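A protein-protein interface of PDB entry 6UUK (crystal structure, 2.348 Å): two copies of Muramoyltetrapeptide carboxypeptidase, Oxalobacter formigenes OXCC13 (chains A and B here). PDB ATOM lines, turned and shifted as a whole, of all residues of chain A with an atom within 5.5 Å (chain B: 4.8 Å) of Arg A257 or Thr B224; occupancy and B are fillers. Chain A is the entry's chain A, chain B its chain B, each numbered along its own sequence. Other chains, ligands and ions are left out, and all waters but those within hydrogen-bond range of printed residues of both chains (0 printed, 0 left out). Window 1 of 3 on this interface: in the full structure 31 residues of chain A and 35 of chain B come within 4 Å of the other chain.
Of the printed residues of chain B, Glu A256 touches Tyr B127 (3.2 Å). Arg A257 touches just these residues of chain B: Thr B224 (3.5 Å), Met B225 (3.4 Å) and His B228 (3.0 Å). Of the printed residues of chain B, Gln A261 touches Ala B227 and His B228. Of chain A, only Arg A257 comes within 4 Å of Thr B224. Leu B226 touches none of the printed residues of chain A. The nearest residue of chain B that does not touch Arg A257 is Tyr B127 (4.03 Å). The nearest printed residue of chain B that does not touch Tyr A253 is Met B225 (6.4 Å).
The side-chain carboxylate (OE2) of Glu A256 lies within hydrogen-bond range of the side-chain hydroxyl (OH) of Tyr B127 (3.2 Å). The backbone carbonyl oxygen of His B228 lies close to the side-chain amide nitrogen of Gln A261, 3.4 Å away. A ring nitrogen (ND1) of His B228 lies close to the backbone carbonyl oxygen (O) of Arg A257 (3.5 Å). The side-chain amide nitrogen (NE2) of Gln A261 lies within hydrogen-bond range of the backbone carbonyl oxygen (O) of Ala B227 (2.8 Å).
Among the printed residues, 8 pairs touch across the chains.
1 position is printed for both chains.
OD1 of Asn B222 sits at hydrogen-bond distance from N of Met B225, at 3.1 Å. The side-chain amide oxygen (OD1) of Asn B222 lies within hydrogen-bond range of the backbone NH (N) of Thr B224, 2.9 Å away. The side-chain sulfur of Met B258 is in hydrogen-bond range of the side-chain hydroxyl of Thr B224 (3.6 Å). NH1 of Arg A254 lies within hydrogen-bond range of OH of Tyr A253 (2.5 Å). The side-chain carboxylate (OD2) of Asp B247 is in hydrogen-bond range of the side-chain hydroxyl (OG1) of Thr B224, 2.5 Å away.
Tyr A253 touches Tyr B127. Thr B224 touches Arg A257. Met B225 touches Arg A257 (CE to NH1, 3.4 Å). Leu A260 touches Tyr B127.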
ATOM      1  N   PRO A 252     -36.068  10.770   3.777  1.00  0.00           N
ATOM      2  CA  PRO A 252     -36.284   9.406   4.293  1.00  0.00           C
ATOM      3  C   PRO A 252     -35.356   8.354   3.703  1.00  0.00           C
ATOM      4  O   PRO A 252     -35.028   7.381   4.395  1.00  0.00           O
ATOM      5  CB  PRO A 252     -37.749   9.140   3.929  1.00  0.00           C
ATOM      6  CG  PRO A 252     -38.382  10.489   3.992  1.00  0.00           C
ATOM      7  CD  PRO A 252     -37.339  11.464   3.506  1.00  0.00           C
ATOM      8  N   TYR A 253     -34.917   8.511   2.452  1.00  0.00           N
ATOM      9  CA  TYR A 253     -33.943   7.573   1.906  1.00  0.00           C
ATOM     10  C   TYR A 253     -32.533   7.876   2.401  1.00  0.00           C
ATOM     11  O   TYR A 253     -31.732   6.951   2.576  1.00  0.00           O
ATOM     12  CB  TYR A 253     -33.992   7.579   0.374  1.00  0.00           C
ATOM     13  CG  TYR A 253     -33.040   8.546  -0.299  1.00  0.00           C
ATOM     14  CD1 TYR A 253     -31.800   8.123  -0.758  1.00  0.00           C
ATOM     15  CD2 TYR A 253     -33.388   9.874  -0.489  1.00  0.00           C
ATOM     16  CE1 TYR A 253     -30.929   9.000  -1.377  1.00  0.00           C
ATOM     17  CE2 TYR A 253     -32.527  10.759  -1.108  1.00  0.00           C
ATOM     18  CZ  TYR A 253     -31.299  10.316  -1.550  1.00  0.00           C
ATOM     19  OH  TYR A 253     -30.437  11.194  -2.167  1.00  0.00           O
ATOM     20  N   ARG A 254     -32.215   9.153   2.630  1.00  0.00           N
ATOM     21  CA  ARG A 254     -30.941   9.492   3.254  1.00  0.00           C
ATOM     22  C   ARG A 254     -30.942   9.145   4.737  1.00  0.00           C
ATOM     23  O   ARG A 254     -29.884   8.853   5.305  1.00  0.00           O
ATOM     24  CB  ARG A 254     -30.631  10.975   3.047  1.00  0.00           C
ATOM     25  CG  ARG A 254     -30.122  11.313   1.654  1.00  0.00           C
ATOM     26  CD  ARG A 254     -29.896  12.809   1.488  1.00  0.00           C
ATOM     27  NE  ARG A 254     -31.064  13.486   0.930  1.00  0.00           N
ATOM     28  CZ  ARG A 254     -31.209  13.780  -0.358  1.00  0.00           C
ATOM     29  NH1 ARG A 254     -30.259  13.460  -1.226  1.00  0.00           N
ATOM     30  NH2 ARG A 254     -32.305  14.398  -0.781  1.00  0.00           N
ATOM     31  N   VAL A 255     -32.113   9.172   5.378  1.00  0.00           N
ATOM     32  CA  VAL A 255     -32.217   8.710   6.757  1.00  0.00           C
ATOM     33  C   VAL A 255     -32.062   7.196   6.821  1.00  0.00           C
ATOM     34  O   VAL A 255     -31.369   6.665   7.698  1.00  0.00           O
ATOM     35  CB  VAL A 255     -33.551   9.173   7.373  1.00  0.00           C
ATOM     36  CG1 VAL A 255     -33.766   8.526   8.733  1.00  0.00           C
ATOM     37  CG2 VAL A 255     -33.583  10.688   7.490  1.00  0.00           C
ATOM     38  N   GLU A 256     -32.698   6.479   5.892  1.00  0.00           N
ATOM     39  CA  GLU A 256     -32.546   5.028   5.841  1.00  0.00           C
ATOM     40  C   GLU A 256     -31.122   4.627   5.479  1.00  0.00           C
ATOM     41  O   GLU A 256     -30.626   3.605   5.964  1.00  0.00           O
ATOM     42  CB  GLU A 256     -33.536   4.434   4.839  1.00  0.00           C
ATOM     43  CG  GLU A 256     -33.449   2.923   4.696  1.00  0.00           C
ATOM     44  CD  GLU A 256     -34.402   2.381   3.651  1.00  0.00           C
ATOM     45  OE1 GLU A 256     -35.458   3.006   3.423  1.00  0.00           O
ATOM     46  OE2 GLU A 256     -34.091   1.329   3.052  1.00  0.00           O
ATOM     47  N   ARG A 257     -30.452   5.418   4.639  1.00  0.00           N
ATOM     48  CA  ARG A 257     -29.088   5.087   4.239  1.00  0.00           C
ATOM     49  C   ARG A 257     -28.126   5.182   5.417  1.00  0.00           C
ATOM     50  O   ARG A 257     -27.268   4.310   5.595  1.00  0.00           O
ATOM     51  CB  ARG A 257     -28.642   6.009   3.103  1.00  0.00           C
ATOM     52  CG  ARG A 257     -27.264   5.697   2.546  1.00  0.00           C
ATOM     53  CD  ARG A 257     -26.912   6.653   1.418  1.00  0.00           C
ATOM     54  NE  ARG A 257     -26.856   8.038   1.878  1.00  0.00           N
ATOM     55  CZ  ARG A 257     -26.761   9.089   1.071  1.00  0.00           C
ATOM     56  NH1 ARG A 257     -26.718   8.918  -0.243  1.00  0.00           N
ATOM     57  NH2 ARG A 257     -26.717  10.314   1.577  1.00  0.00           N
ATOM     58  N   MET A 258     -28.254   6.224   6.231  1.00  0.00           N
ATOM     59  CA  MET A 258     -27.369   6.413   7.373  1.00  0.00           C
ATOM     60  C   MET A 258     -27.655   5.402   8.480  1.00  0.00           C
ATOM     61  O   MET A 258     -26.753   5.016   9.225  1.00  0.00           O
ATOM     62  CB  MET A 258     -27.493   7.837   7.912  1.00  0.00           C
ATOM     63  CG  MET A 258     -26.991   8.899   6.950  1.00  0.00           C
ATOM     64  SD  MET A 258     -27.152  10.704   7.659  1.00  0.00           S
ATOM     65  CE  MET A 258     -26.289  11.678   6.207  1.00  0.00           C
ATOM     66  N   LEU A 259     -28.915   4.974   8.585  1.00  0.00           N
ATOM     67  CA  LEU A 259     -29.262   3.950   9.565  1.00  0.00           C
ATOM     68  C   LEU A 259     -28.761   2.577   9.142  1.00  0.00           C
ATOM     69  O   LEU A 259     -28.462   1.737   9.998  1.00  0.00           O
ATOM     70  CB  LEU A 259     -30.774   3.923   9.788  1.00  0.00           C
ATOM     71  CG  LEU A 259     -31.330   5.002  10.718  1.00  0.00           C
ATOM     72  CD1 LEU A 259     -32.849   5.004  10.697  1.00  0.00           C
ATOM     73  CD2 LEU A 259     -30.814   4.797  12.134  1.00  0.00           C
ATOM     74  N   LEU A 260     -28.662   2.328   7.834  1.00  0.00           N
ATOM     75  CA  LEU A 260     -28.117   1.058   7.367  1.00  0.00           C
ATOM     76  C   LEU A 260     -26.608   0.990   7.561  1.00  0.00           C
ATOM     77  O   LEU A 260     -26.055  -0.105   7.715  1.00  0.00           O
ATOM     78  CB  LEU A 260     -28.476   0.837   5.898  1.00  0.00           C
ATOM     79  CG  LEU A 260     -29.930   0.456   5.615  1.00  0.00           C
ATOM     80  CD1 LEU A 260     -30.208   0.463   4.122  1.00  0.00           C
ATOM     81  CD2 LEU A 260     -30.250  -0.906   6.214  1.00  0.00           C
ATOM     82  N   GLN A 261     -25.929   2.140   7.556  1.00  0.00           N
ATOM     83  CA  GLN A 261     -24.495   2.150   7.827  1.00  0.00           C
ATOM     84  C   GLN A 261     -24.201   1.652   9.236  1.00  0.00           C
ATOM     85  O   GLN A 261     -23.281   0.851   9.440  1.00  0.00           O
ATOM     86  CB  GLN A 261     -23.929   3.557   7.630  1.00  0.00           C
ATOM     87  CG  GLN A 261     -22.454   3.684   7.979  1.00  0.00           C
ATOM     88  CD  GLN A 261     -21.899   5.060   7.678  1.00  0.00           C
ATOM     89  OE1 GLN A 261     -22.644   5.989   7.366  1.00  0.00           O
ATOM     90  NE2 GLN A 261     -20.580   5.200   7.764  1.00  0.00           N
ATOM     91  N   TYR B 127     -29.941   5.809  -5.203  1.00  0.00           N
ATOM     92  CA  TYR B 127     -30.454   4.944  -4.140  1.00  0.00           C
ATOM     93  C   TYR B 127     -31.878   4.474  -4.432  1.00  0.00           C
ATOM     94  O   TYR B 127     -32.332   4.500  -5.575  1.00  0.00           O
ATOM     95  CB  TYR B 127     -30.401   5.668  -2.790  1.00  0.00           C
ATOM     96  CG  TYR B 127     -30.654   4.783  -1.589  1.00  0.00           C
ATOM     97  CD1 TYR B 127     -29.597   4.242  -0.869  1.00  0.00           C
ATOM     98  CD2 TYR B 127     -31.947   4.499  -1.168  1.00  0.00           C
ATOM     99  CE1 TYR B 127     -29.822   3.436   0.233  1.00  0.00           C
ATOM    100  CE2 TYR B 127     -32.181   3.694  -0.069  1.00  0.00           C
ATOM    101  CZ  TYR B 127     -31.115   3.167   0.627  1.00  0.00           C
ATOM    102  OH  TYR B 127     -31.343   2.366   1.723  1.00  0.00           O
ATOM    103  N   ASN B 222     -17.734   7.658  -5.278  1.00  0.00           N
ATOM    104  CA  ASN B 222     -18.524   8.726  -4.683  1.00  0.00           C
ATOM    105  C   ASN B 222     -18.151   8.894  -3.215  1.00  0.00           C
ATOM    106  O   ASN B 222     -18.059   7.912  -2.473  1.00  0.00           O
ATOM    107  CB  ASN B 222     -20.015   8.426  -4.827  1.00  0.00           C
ATOM    108  CG  ASN B 222     -20.889   9.549  -4.307  1.00  0.00           C
ATOM    109  OD1 ASN B 222     -21.317   9.532  -3.155  1.00  0.00           O
ATOM    110  ND2 ASN B 222     -21.157  10.533  -5.157  1.00  0.00           N
ATOM    111  N   LEU B 223     -17.938  10.146  -2.799  1.00  0.00           N
ATOM    112  CA  LEU B 223     -17.488  10.404  -1.433  1.00  0.00           C
ATOM    113  C   LEU B 223     -18.557  10.037  -0.411  1.00  0.00           C
ATOM    114  O   LEU B 223     -18.239   9.527   0.670  1.00  0.00           O
ATOM    115  CB  LEU B 223     -17.084  11.870  -1.284  1.00  0.00           C
ATOM    116  CG  LEU B 223     -16.616  12.300   0.109  1.00  0.00           C
ATOM    117  CD1 LEU B 223     -15.410  11.483   0.549  1.00  0.00           C
ATOM    118  CD2 LEU B 223     -16.301  13.785   0.137  1.00  0.00           C
ATOM    119  N   THR B 224     -19.828  10.289  -0.731  1.00  0.00           N
ATOM    120  CA  THR B 224     -20.899   9.967   0.206  1.00  0.00           C
ATOM    121  C   THR B 224     -21.039   8.460   0.387  1.00  0.00           C
ATOM    122  O   THR B 224     -21.308   7.983   1.496  1.00  0.00           O
ATOM    123  CB  THR B 224     -22.218  10.578  -0.270  1.00  0.00           C
ATOM    124  OG1 THR B 224     -22.056  11.992  -0.442  1.00  0.00           O
ATOM    125  CG2 THR B 224     -23.327  10.323   0.740  1.00  0.00           C
ATOM    126  N   MET B 225     -20.848   7.697  -0.684  1.00  0.00           N
ATOM    127  CA  MET B 225     -20.982   6.247  -0.621  1.00  0.00           C
ATOM    128  C   MET B 225     -19.765   5.604   0.036  1.00  0.00           C
ATOM    129  O   MET B 225     -19.869   4.537   0.639  1.00  0.00           O
ATOM    130  CB  MET B 225     -21.196   5.670  -2.021  1.00  0.00           C
ATOM    131  CG  MET B 225     -22.277   6.385  -2.811  1.00  0.00           C
ATOM    132  SD  MET B 225     -23.964   6.500  -1.840  1.00  0.00           S
ATOM    133  CE  MET B 225     -24.844   7.860  -2.927  1.00  0.00           C
ATOM    134  N   LEU B 226     -18.608   6.259  -0.083  1.00  0.00           N
ATOM    135  CA  LEU B 226     -17.402   5.751   0.562  1.00  0.00           C
ATOM    136  C   LEU B 226     -17.429   6.002   2.065  1.00  0.00           C
ATOM    137  O   LEU B 226     -17.093   5.113   2.855  1.00  0.00           O
ATOM    138  CB  LEU B 226     -16.160   6.380  -0.070  1.00  0.00           C
ATOM    139  CG  LEU B 226     -15.781   5.858  -1.456  1.00  0.00           C
ATOM    140  CD1 LEU B 226     -14.557   6.582  -1.991  1.00  0.00           C
ATOM    141  CD2 LEU B 226     -15.544   4.357  -1.413  1.00  0.00           C
ATOM    142  N   ALA B 227     -17.821   7.212   2.478  1.00  0.00           N
ATOM    143  CA  ALA B 227     -18.000   7.476   3.902  1.00  0.00           C
ATOM    144  C   ALA B 227     -19.121   6.625   4.483  1.00  0.00           C
ATOM    145  O   ALA B 227     -19.090   6.280   5.669  1.00  0.00           O
ATOM    146  CB  ALA B 227     -18.281   8.961   4.130  1.00  0.00           C
ATOM    147  N   HIS B 228     -20.114   6.280   3.661  1.00  0.00           N
ATOM    148  CA  HIS B 228     -21.144   5.331   4.069  1.00  0.00           C
ATOM    149  C   HIS B 228     -20.579   3.935   4.300  1.00  0.00           C
ATOM    150  O   HIS B 228     -21.164   3.158   5.063  1.00  0.00           O
ATOM    151  CB  HIS B 228     -22.252   5.289   3.012  1.00  0.00           C
ATOM    152  CG  HIS B 228     -23.266   4.212   3.234  1.00  0.00           C
ATOM    153  ND1 HIS B 228     -24.020   4.123   4.384  1.00  0.00           N
ATOM    154  CD2 HIS B 228     -23.655   3.180   2.448  1.00  0.00           C
ATOM    155  CE1 HIS B 228     -24.827   3.080   4.298  1.00  0.00           C
ATOM    156  NE2 HIS B 228     -24.626   2.492   3.134  1.00  0.00           N
ATOM    157  N   ASP B 247     -18.115  14.099  -5.653  1.00  0.00           N
ATOM    158  CA  ASP B 247     -19.441  14.302  -5.081  1.00  0.00           C
ATOM    159  C   ASP B 247     -20.078  15.521  -5.735  1.00  0.00           C
ATOM    160  O   ASP B 247     -19.425  16.276  -6.459  1.00  0.00           O
ATOM    161  CB  ASP B 247     -19.374  14.475  -3.561  1.00  0.00           C
ATOM    162  CG  ASP B 247     -20.500  13.760  -2.843  1.00  0.00           C
ATOM    163  OD1 ASP B 247     -21.573  13.572  -3.453  1.00  0.00           O
ATOM    164  OD2 ASP B 247     -20.310  13.384  -1.667  1.00  0.00           O
ATOM    165  N   GLU B 250     -22.623  19.195  -2.438  1.00  0.00           N
ATOM    166  CA  GLU B 250     -21.966  19.147  -1.138  1.00  0.00           C
ATOM    167  C   GLU B 250     -21.191  20.434  -0.904  1.00  0.00           C
ATOM    168  O   GLU B 250     -20.314  20.788  -1.698  1.00  0.00           O
ATOM    169  CB  GLU B 250     -21.030  17.941  -1.036  1.00  0.00           C
ATOM    170  CG  GLU B 250     -21.708  16.606  -1.277  1.00  0.00           C
ATOM    171  CD  GLU B 250     -22.874  16.361  -0.340  1.00  0.00           C
ATOM    172  OE1 GLU B 250     -22.770  16.712   0.853  1.00  0.00           O
ATOM    173  OE2 GLU B 250     -23.900  15.820  -0.803  1.00  0.00           O
ATOM    174  N   MET B 258     -16.746  14.199   5.556  1.00  0.00           N
ATOM    175  CA  MET B 258     -16.680  12.816   5.099  1.00  0.00           C
ATOM    176  C   MET B 258     -15.240  12.369   4.870  1.00  0.00           C
ATOM    177  O   MET B 258     -14.918  11.189   5.011  1.00  0.00           O
ATOM    178  CB  MET B 258     -17.504  12.639   3.825  1.00  0.00           C
ATOM    179  CG  MET B 258     -18.997  12.815   4.045  1.00  0.00           C
ATOM    180  SD  MET B 258     -20.042  12.692   2.406  1.00  0.00           S
ATOM    181  CE  MET B 258     -21.827  12.756   3.187  1.00  0.00           C
